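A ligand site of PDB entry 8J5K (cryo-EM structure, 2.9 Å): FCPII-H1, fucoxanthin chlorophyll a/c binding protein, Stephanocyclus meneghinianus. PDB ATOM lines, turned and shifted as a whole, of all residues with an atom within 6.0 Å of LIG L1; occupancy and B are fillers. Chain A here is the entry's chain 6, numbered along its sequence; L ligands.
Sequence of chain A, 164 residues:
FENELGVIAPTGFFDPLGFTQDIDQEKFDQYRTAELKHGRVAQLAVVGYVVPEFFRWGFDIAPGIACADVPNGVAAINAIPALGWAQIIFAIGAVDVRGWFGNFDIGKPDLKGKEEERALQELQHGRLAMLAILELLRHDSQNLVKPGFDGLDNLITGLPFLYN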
ATOM      1  N   ILE A  61     -32.557  30.024  23.294  1.00  0.00           N
ATOM      2  CA  ILE A  61     -31.193  30.075  23.795  1.00  0.00           C
ATOM      3  C   ILE A  61     -30.880  31.503  24.213  1.00  0.00           C
ATOM      4  O   ILE A  61     -31.253  32.463  23.524  1.00  0.00           O
ATOM      5  CB  ILE A  61     -30.200  29.579  22.744  1.00  0.00           C
ATOM      6  N   ALA A  62     -30.229  31.647  25.377  1.00  0.00           N
ATOM      7  CA  ALA A  62     -29.869  32.935  25.976  1.00  0.00           C
ATOM      8  C   ALA A  62     -31.104  33.664  26.481  1.00  0.00           C
ATOM      9  O   ALA A  62     -32.235  33.291  26.125  1.00  0.00           O
ATOM     10  CB  ALA A  62     -29.095  33.794  24.973  1.00  0.00           C
ATOM     11  N   PRO A  63     -30.942  34.691  27.341  1.00  0.00           N
ATOM     12  CA  PRO A  63     -32.106  35.442  27.850  1.00  0.00           C
ATOM     13  C   PRO A  63     -33.135  35.816  26.793  1.00  0.00           C
ATOM     14  O   PRO A  63     -34.313  35.460  26.923  1.00  0.00           O
ATOM     15  CB  PRO A  63     -31.471  36.688  28.461  1.00  0.00           C
ATOM     16  CG  PRO A  63     -30.096  36.258  28.865  1.00  0.00           C
ATOM     17  CD  PRO A  63     -29.715  35.045  28.068  1.00  0.00           C
ATOM     18  N   ILE A  80     -24.512  34.557  20.578  1.00  0.00           N
ATOM     19  CA  ILE A  80     -24.946  33.875  21.797  1.00  0.00           C
ATOM     20  C   ILE A  80     -24.059  34.368  22.937  1.00  0.00           C
ATOM     21  O   ILE A  80     -22.831  34.342  22.802  1.00  0.00           O
ATOM     22  CB  ILE A  80     -24.859  32.340  21.663  1.00  0.00           C
ATOM     23  CG1 ILE A  80     -26.022  31.826  20.820  1.00  0.00           C
ATOM     24  CG2 ILE A  80     -24.870  31.683  23.021  1.00  0.00           C
ATOM     25  CD1 ILE A  80     -26.000  30.324  20.598  1.00  0.00           C
ATOM     26  N   PRO A  81     -24.642  34.836  24.048  1.00  0.00           N
ATOM     27  CA  PRO A  81     -23.836  35.333  25.168  1.00  0.00           C
ATOM     28  C   PRO A  81     -22.695  34.393  25.534  1.00  0.00           C
ATOM     29  O   PRO A  81     -22.835  33.172  25.517  1.00  0.00           O
ATOM     30  CB  PRO A  81     -24.859  35.444  26.295  1.00  0.00           C
ATOM     31  CG  PRO A  81     -26.141  35.766  25.594  1.00  0.00           C
ATOM     32  CD  PRO A  81     -26.057  35.196  24.194  1.00  0.00           C
ATOM     33  N   ALA A  82     -21.552  34.992  25.886  1.00  0.00           N
ATOM     34  CA  ALA A  82     -20.338  34.230  26.111  1.00  0.00           C
ATOM     35  C   ALA A  82     -20.474  33.241  27.252  1.00  0.00           C
ATOM     36  O   ALA A  82     -19.855  32.167  27.221  1.00  0.00           O
ATOM     37  CB  ALA A  82     -19.168  35.187  26.382  1.00  0.00           C
ATOM     38  N   LEU A  83     -21.274  33.569  28.263  1.00  0.00           N
ATOM     39  CA  LEU A  83     -21.452  32.646  29.386  1.00  0.00           C
ATOM     40  C   LEU A  83     -22.099  31.346  28.918  1.00  0.00           C
ATOM     41  O   LEU A  83     -21.676  30.256  29.325  1.00  0.00           O
ATOM     42  CB  LEU A  83     -22.292  33.309  30.474  1.00  0.00           C
ATOM     43  CG  LEU A  83     -22.143  32.743  31.884  1.00  0.00           C
ATOM     44  CD1 LEU A  83     -20.679  32.518  32.212  1.00  0.00           C
ATOM     45  CD2 LEU A  83     -22.777  33.688  32.903  1.00  0.00           C
ATOM     46  N   GLY A  84     -23.110  31.433  28.059  1.00  0.00           N
ATOM     47  CA  GLY A  84     -23.733  30.231  27.537  1.00  0.00           C
ATOM     48  C   GLY A  84     -22.773  29.378  26.723  1.00  0.00           C
ATOM     49  O   GLY A  84     -22.764  28.152  26.832  1.00  0.00           O
ATOM     50  N   TRP A  85     -21.952  30.034  25.890  1.00  0.00           N
ATOM     51  CA  TRP A  85     -20.964  29.294  25.114  1.00  0.00           C
ATOM     52  C   TRP A  85     -19.960  28.598  26.027  1.00  0.00           C
ATOM     53  O   TRP A  85     -19.591  27.442  25.784  1.00  0.00           O
ATOM     54  CB  TRP A  85     -20.246  30.236  24.147  1.00  0.00           C
ATOM     55  CG  TRP A  85     -20.817  30.229  22.767  1.00  0.00           C
ATOM     56  CD1 TRP A  85     -21.343  31.292  22.099  1.00  0.00           C
ATOM     57  CD2 TRP A  85     -20.911  29.114  21.877  1.00  0.00           C
ATOM     58  NE1 TRP A  85     -21.766  30.906  20.856  1.00  0.00           N
ATOM     59  CE2 TRP A  85     -21.509  29.567  20.690  1.00  0.00           C
ATOM     60  CE3 TRP A  85     -20.553  27.765  21.975  1.00  0.00           C
ATOM     61  CZ2 TRP A  85     -21.766  28.736  19.612  1.00  0.00           C
ATOM     62  CZ3 TRP A  85     -20.793  26.932  20.896  1.00  0.00           C
ATOM     63  CH2 TRP A  85     -21.398  27.424  19.735  1.00  0.00           C
ATOM     64  N   GLN A  87     -20.484  27.588  29.107  1.00  0.00           N
ATOM     65  CA  GLN A  87     -21.150  26.462  29.772  1.00  0.00           C
ATOM     66  C   GLN A  87     -21.293  25.278  28.825  1.00  0.00           C
ATOM     67  O   GLN A  87     -21.094  24.133  29.240  1.00  0.00           O
ATOM     68  CB  GLN A  87     -22.500  26.909  30.310  1.00  0.00           C
ATOM     69  CG  GLN A  87     -22.384  28.022  31.325  1.00  0.00           C
ATOM     70  CD  GLN A  87     -23.700  28.715  31.571  1.00  0.00           C
ATOM     71  OE1 GLN A  87     -23.939  29.828  31.087  1.00  0.00           O
ATOM     72  NE2 GLN A  87     -24.561  28.081  32.355  1.00  0.00           N
ATOM     73  N   ILE A  88     -21.637  25.530  27.560  1.00  0.00           N
ATOM     74  CA  ILE A  88     -21.702  24.447  26.585  1.00  0.00           C
ATOM     75  C   ILE A  88     -20.333  23.801  26.432  1.00  0.00           C
ATOM     76  O   ILE A  88     -20.215  22.566  26.346  1.00  0.00           O
ATOM     77  CB  ILE A  88     -22.236  24.968  25.232  1.00  0.00           C
ATOM     78  CG1 ILE A  88     -23.661  25.481  25.384  1.00  0.00           C
ATOM     79  CG2 ILE A  88     -22.171  23.875  24.186  1.00  0.00           C
ATOM     80  CD1 ILE A  88     -24.149  26.237  24.164  1.00  0.00           C
ATOM     81  N   ALA A  91     -19.627  21.617  29.434  1.00  0.00           N
ATOM     82  CA  ALA A  91     -20.450  20.403  29.423  1.00  0.00           C
ATOM     83  C   ALA A  91     -19.909  19.382  28.425  1.00  0.00           C
ATOM     84  O   ALA A  91     -19.833  18.182  28.745  1.00  0.00           O
ATOM     85  CB  ALA A  91     -21.898  20.758  29.091  1.00  0.00           C
HETATM   86 MG1  LIG L   1     -27.372  27.654  31.954  1.00  0.00          MG
HETATM   87  C1  LIG L   1     -27.546  30.679  30.272  1.00  0.00           C
HETATM   88  C2  LIG L   1     -27.980  29.259  34.895  1.00  0.00           C
HETATM   89  C3  LIG L   1     -27.212  24.630  33.578  1.00  0.00           C
HETATM   90  C4  LIG L   1     -26.659  26.046  28.890  1.00  0.00           C
HETATM   91  N1  LIG L   1     -27.717  29.650  32.464  1.00  0.00           N
HETATM   92  C5  LIG L   1     -27.752  30.769  31.619  1.00  0.00           C
HETATM   93  C6  LIG L   1     -28.030  32.047  32.412  1.00  0.00           C
HETATM   94  C7  LIG L   1     -28.092  31.568  33.874  1.00  0.00           C
HETATM   95  C8  LIG L   1     -27.928  30.051  33.761  1.00  0.00           C
HETATM   96  C9  LIG L   1     -27.003  32.179  34.707  1.00  0.00           C
HETATM   97  C10 LIG L   1     -29.350  32.652  31.990  1.00  0.00           C
HETATM   98  C11 LIG L   1     -29.271  34.156  31.938  1.00  0.00           C
HETATM   99  C12 LIG L   1     -29.265  34.697  33.335  1.00  0.00           C
HETATM  100  O1  LIG L   1     -28.624  35.651  33.791  1.00  0.00           O
HETATM  101  O2  LIG L   1     -30.100  34.007  34.164  1.00  0.00           O
HETATM  102  N2  LIG L   1     -27.552  27.054  33.867  1.00  0.00           N
HETATM  103  C13 LIG L   1     -27.819  27.864  34.922  1.00  0.00           C
HETATM  104  C14 LIG L   1     -27.922  27.045  36.165  1.00  0.00           C
HETATM  105  C15 LIG L   1     -27.708  25.734  35.800  1.00  0.00           C
HETATM  106  C16 LIG L   1     -27.471  25.726  34.330  1.00  0.00           C
HETATM  107  C17 LIG L   1     -28.193  27.620  37.485  1.00  0.00           C
HETATM  108  C18 LIG L   1     -27.692  24.544  36.609  1.00  0.00           C
HETATM  109  N3  LIG L   1     -27.016  25.697  31.335  1.00  0.00           N
HETATM  110  C19 LIG L   1     -26.997  24.612  32.164  1.00  0.00           C
HETATM  111  C20 LIG L   1     -26.712  23.407  31.399  1.00  0.00           C
HETATM  112  C21 LIG L   1     -26.553  23.803  30.076  1.00  0.00           C
HETATM  113  C22 LIG L   1     -26.745  25.248  30.036  1.00  0.00           C
HETATM  114  C23 LIG L   1     -26.623  22.063  31.963  1.00  0.00           C
HETATM  115  C24 LIG L   1     -26.248  22.940  28.917  1.00  0.00           C
HETATM  116  C25 LIG L   1     -24.788  23.007  28.540  1.00  0.00           C
HETATM  117  N4  LIG L   1     -27.172  28.164  30.016  1.00  0.00           N
HETATM  118  C26 LIG L   1     -26.863  27.412  28.852  1.00  0.00           C
HETATM  119  C27 LIG L   1     -26.797  28.326  27.686  1.00  0.00           C
HETATM  120  C28 LIG L   1     -27.062  29.591  28.179  1.00  0.00           C
HETATM  121  C29 LIG L   1     -27.279  29.434  29.625  1.00  0.00           C
HETATM  122  C30 LIG L   1     -26.507  27.919  26.321  1.00  0.00           C
HETATM  123  C31 LIG L   1     -27.197  30.994  27.852  1.00  0.00           C
HETATM  124  O3  LIG L   1     -27.099  31.551  26.772  1.00  0.00           O
HETATM  125  C32 LIG L   1     -27.494  31.741  29.195  1.00  0.00           C
HETATM  126  C33 LIG L   1     -26.430  32.751  29.499  1.00  0.00           C
HETATM  127  O4  LIG L   1     -25.298  32.539  29.931  1.00  0.00           O
HETATM  128  O5  LIG L   1     -26.803  34.039  29.258  1.00  0.00           O
HETATM  129  C34 LIG L   1     -26.107  35.060  29.972  1.00  0.00           C
HETATM  130  C1  LG2 L   2     -27.952  22.276  25.609  1.00  0.00           C
HETATM  131  O1  LG2 L   2     -18.798  15.965  19.168  1.00  0.00           O
HETATM  132  C2  LG2 L   2     -27.524  23.490  24.841  1.00  0.00           C
HETATM  133  C3  LG2 L   2     -21.213  17.617  20.899  1.00  0.00           C
HETATM  134  C4  LG2 L   2     -19.988  17.556  20.375  1.00  0.00           C
HETATM  135  C5  LG2 L   2     -19.338  18.825  19.919  1.00  0.00           C
HETATM  136  C6  LG2 L   2     -19.283  16.298  20.226  1.00  0.00           C
HETATM  137  C7  LG2 L   2     -19.212  15.416  21.456  1.00  0.00           C
HETATM  138  C8  LG2 L   2     -18.257  14.236  21.283  1.00  0.00           C
HETATM  139  C9  LG2 L   2     -16.824  14.593  21.723  1.00  0.00           C
HETATM  140  C10 LG2 L   2     -15.756  13.530  21.538  1.00  0.00           C
HETATM  141  C11 LG2 L   2     -16.208  12.308  22.286  1.00  0.00           C
HETATM  142  C12 LG2 L   2     -17.434  11.739  21.611  1.00  0.00           C
HETATM  143  C13 LG2 L   2     -26.582  23.404  23.897  1.00  0.00           C
HETATM  144  C14 LG2 L   2     -18.545  12.740  21.314  1.00  0.00           C
HETATM  145  C15 LG2 L   2     -19.736  12.214  20.535  1.00  0.00           C
HETATM  146  C16 LG2 L   2     -16.916  14.880  23.218  1.00  0.00           C
HETATM  147  C17 LG2 L   2     -16.281  15.885  21.110  1.00  0.00           C
HETATM  148  C18 LG2 L   2     -28.111  24.806  25.107  1.00  0.00           C
HETATM  149  C19 LG2 L   2     -29.028  24.933  26.053  1.00  0.00           C
HETATM  150  C20 LG2 L   2     -29.563  26.275  26.249  1.00  0.00           C
HETATM  151  C21 LG2 L   2     -30.478  26.489  27.197  1.00  0.00           C
HETATM  152  C22 LG2 L   2     -30.970  25.359  28.068  1.00  0.00           C
HETATM  153  C23 LG2 L   2     -30.993  27.877  27.340  1.00  0.00           C
HETATM  154  C24 LG2 L   2     -25.999  22.110  23.632  1.00  0.00           C
HETATM  155  C25 LG2 L   2     -31.857  28.113  28.205  1.00  0.00           C
HETATM  156  C26 LG2 L   2     -32.730  28.369  29.079  1.00  0.00           C
HETATM  157  C27 LG2 L   2     -32.238  28.675  30.491  1.00  0.00           C
HETATM  158  C28 LG2 L   2     -33.320  28.379  31.509  1.00  0.00           C
HETATM  159  C29 LG2 L   2     -34.512  29.264  31.149  1.00  0.00           C
HETATM  160  C30 LG2 L   2     -34.993  28.687  29.834  1.00  0.00           C
HETATM  161  C31 LG2 L   2     -34.067  28.849  28.636  1.00  0.00           C
HETATM  162  C32 LG2 L   2     -34.541  28.033  27.447  1.00  0.00           C
HETATM  163  C33 LG2 L   2     -36.814  29.727  31.950  1.00  0.00           C
HETATM  164  C34 LG2 L   2     -37.252  30.726  32.979  1.00  0.00           C
HETATM  165  C35 LG2 L   2     -25.020  22.004  22.757  1.00  0.00           C
HETATM  166  C36 LG2 L   2     -31.841  30.138  30.531  1.00  0.00           C
HETATM  167  C37 LG2 L   2     -31.022  27.829  30.801  1.00  0.00           C
HETATM  168  C38 LG2 L   2     -24.473  20.670  22.559  1.00  0.00           C
HETATM  169  C39 LG2 L   2     -23.423  20.487  21.771  1.00  0.00           C
HETATM  170  C40 LG2 L   2     -22.787  21.624  21.038  1.00  0.00           C
HETATM  171  C41 LG2 L   2     -22.906  19.117  21.644  1.00  0.00           C
HETATM  172  C42 LG2 L   2     -21.769  18.945  21.004  1.00  0.00           C
HETATM  173  O2  LG2 L   2     -18.862  13.557  22.422  1.00  0.00           O
HETATM  174  O3  LG2 L   2     -15.158  11.331  22.239  1.00  0.00           O
HETATM  175  O4  LG2 L   2     -33.951  30.223  28.245  1.00  0.00           O
HETATM  176  O5  LG2 L   2     -35.516  29.073  32.152  1.00  0.00           O
HETATM  177  O6  LG2 L   2     -37.531  29.463  30.990  1.00  0.00           O
HETATM  178 MG1  LG3 L   3     -25.279  11.395  25.126  1.00  0.00          MG
HETATM  179  C1  LG3 L   3     -24.533   8.386  23.572  1.00  0.00           C
HETATM  180  C2  LG3 L   3     -22.422  12.752  23.883  1.00  0.00           C
HETATM  181  C3  LG3 L   3     -26.053  14.339  26.725  1.00  0.00           C
HETATM  182  C4  LG3 L   3     -28.167   9.901  26.510  1.00  0.00           C
HETATM  183  N1  LG3 L   3     -23.754  10.666  23.902  1.00  0.00           N
HETATM  184  C5  LG3 L   3     -23.625   9.388  23.361  1.00  0.00           C
HETATM  185  C6  LG3 L   3     -22.361   9.278  22.524  1.00  0.00           C
HETATM  186  C7  LG3 L   3     -21.660  10.629  22.744  1.00  0.00           C
HETATM  187  C8  LG3 L   3     -22.678  11.431  23.547  1.00  0.00           C
HETATM  188  C9  LG3 L   3     -20.381  10.448  23.528  1.00  0.00           C
HETATM  189  C10 LG3 L   3     -22.733   9.119  21.061  1.00  0.00           C
HETATM  190  N2  LG3 L   3     -24.405  13.200  25.271  1.00  0.00           N
HETATM  191  C11 LG3 L   3     -23.270  13.577  24.648  1.00  0.00           C
HETATM  192  C12 LG3 L   3     -22.994  15.026  24.920  1.00  0.00           C
HETATM  193  C13 LG3 L   3     -24.017  15.472  25.722  1.00  0.00           C
HETATM  194  C14 LG3 L   3     -24.925  14.320  25.957  1.00  0.00           C
HETATM  195  C15 LG3 L   3     -21.820  15.716  24.376  1.00  0.00           C
HETATM  196  C16 LG3 L   3     -24.283  16.761  26.304  1.00  0.00           C
HETATM  197  C17 LG3 L   3     -23.866  17.942  25.844  1.00  0.00           C
HETATM  198  N3  LG3 L   3     -26.838  11.999  26.369  1.00  0.00           N
HETATM  199  C18 LG3 L   3     -26.951  13.253  26.916  1.00  0.00           C
HETATM  200  C19 LG3 L   3     -28.148  13.330  27.745  1.00  0.00           C
HETATM  201  C20 LG3 L   3     -28.749  12.076  27.697  1.00  0.00           C
HETATM  202  C21 LG3 L   3     -27.921  11.247  26.831  1.00  0.00           C
HETATM  203  C22 LG3 L   3     -28.591  14.521  28.470  1.00  0.00           C
HETATM  204  C23 LG3 L   3     -29.984  11.661  28.367  1.00  0.00           C
HETATM  205  C24 LG3 L   3     -31.188  11.737  27.471  1.00  0.00           C
HETATM  206  N4  LG3 L   3     -26.220   9.603  25.048  1.00  0.00           N
HETATM  207  C25 LG3 L   3     -27.398   9.118  25.685  1.00  0.00           C
HETATM  208  C26 LG3 L   3     -27.582   7.699  25.309  1.00  0.00           C
HETATM  209  C27 LG3 L   3     -26.515   7.375  24.497  1.00  0.00           C
HETATM  210  C28 LG3 L   3     -25.697   8.588  24.382  1.00  0.00           C
HETATM  211  C29 LG3 L   3     -28.697   6.860  25.748  1.00  0.00           C
HETATM  212  C30 LG3 L   3     -25.871   6.331  23.715  1.00  0.00           C
HETATM  213  O1  LG3 L   3     -26.231   5.183  23.495  1.00  0.00           O
HETATM  214  C31 LG3 L   3     -24.553   6.944  23.134  1.00  0.00           C
HETATM  215  C32 LG3 L   3     -23.346   6.198  23.614  1.00  0.00           C
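OE1 of Gln 87 lies close to O4 of LIG L1, 3.2 Å away. An oxygen (O4) of LIG L1 sits at hydrogen-bond distance from the backbone NH (N) of Gly 84 (3.1 Å). The backbone NH (N) of Ala 62 lies close to an oxygen (O3) of LIG L1, 3.4 Å away.
OE1 of Gln 87 lies close to O of Leu 83, at 2.9 Å.
Residues that only touch LIG L1: Pro 63 (3.3 Å), Pro 81 (3.8 Å), Leu 83 (3.2 Å), Ile 88 (3.6 Å) and Ala 91 (3.7 Å). Hydrophobic or aromatic side chains that line LIG L1: Ala 62, Pro 63, Pro 81, Leu 83, Ile 88 and Ala 91. Eight residues have an atom within 4 Å of LIG L1: Ala 62, Pro 63, Pro 81, Leu 83, Gly 84, Gln 87, Ile 88 and Ala 91. Along chain A the residues within 4 Å of LIG L1 span positions 62 to 91.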
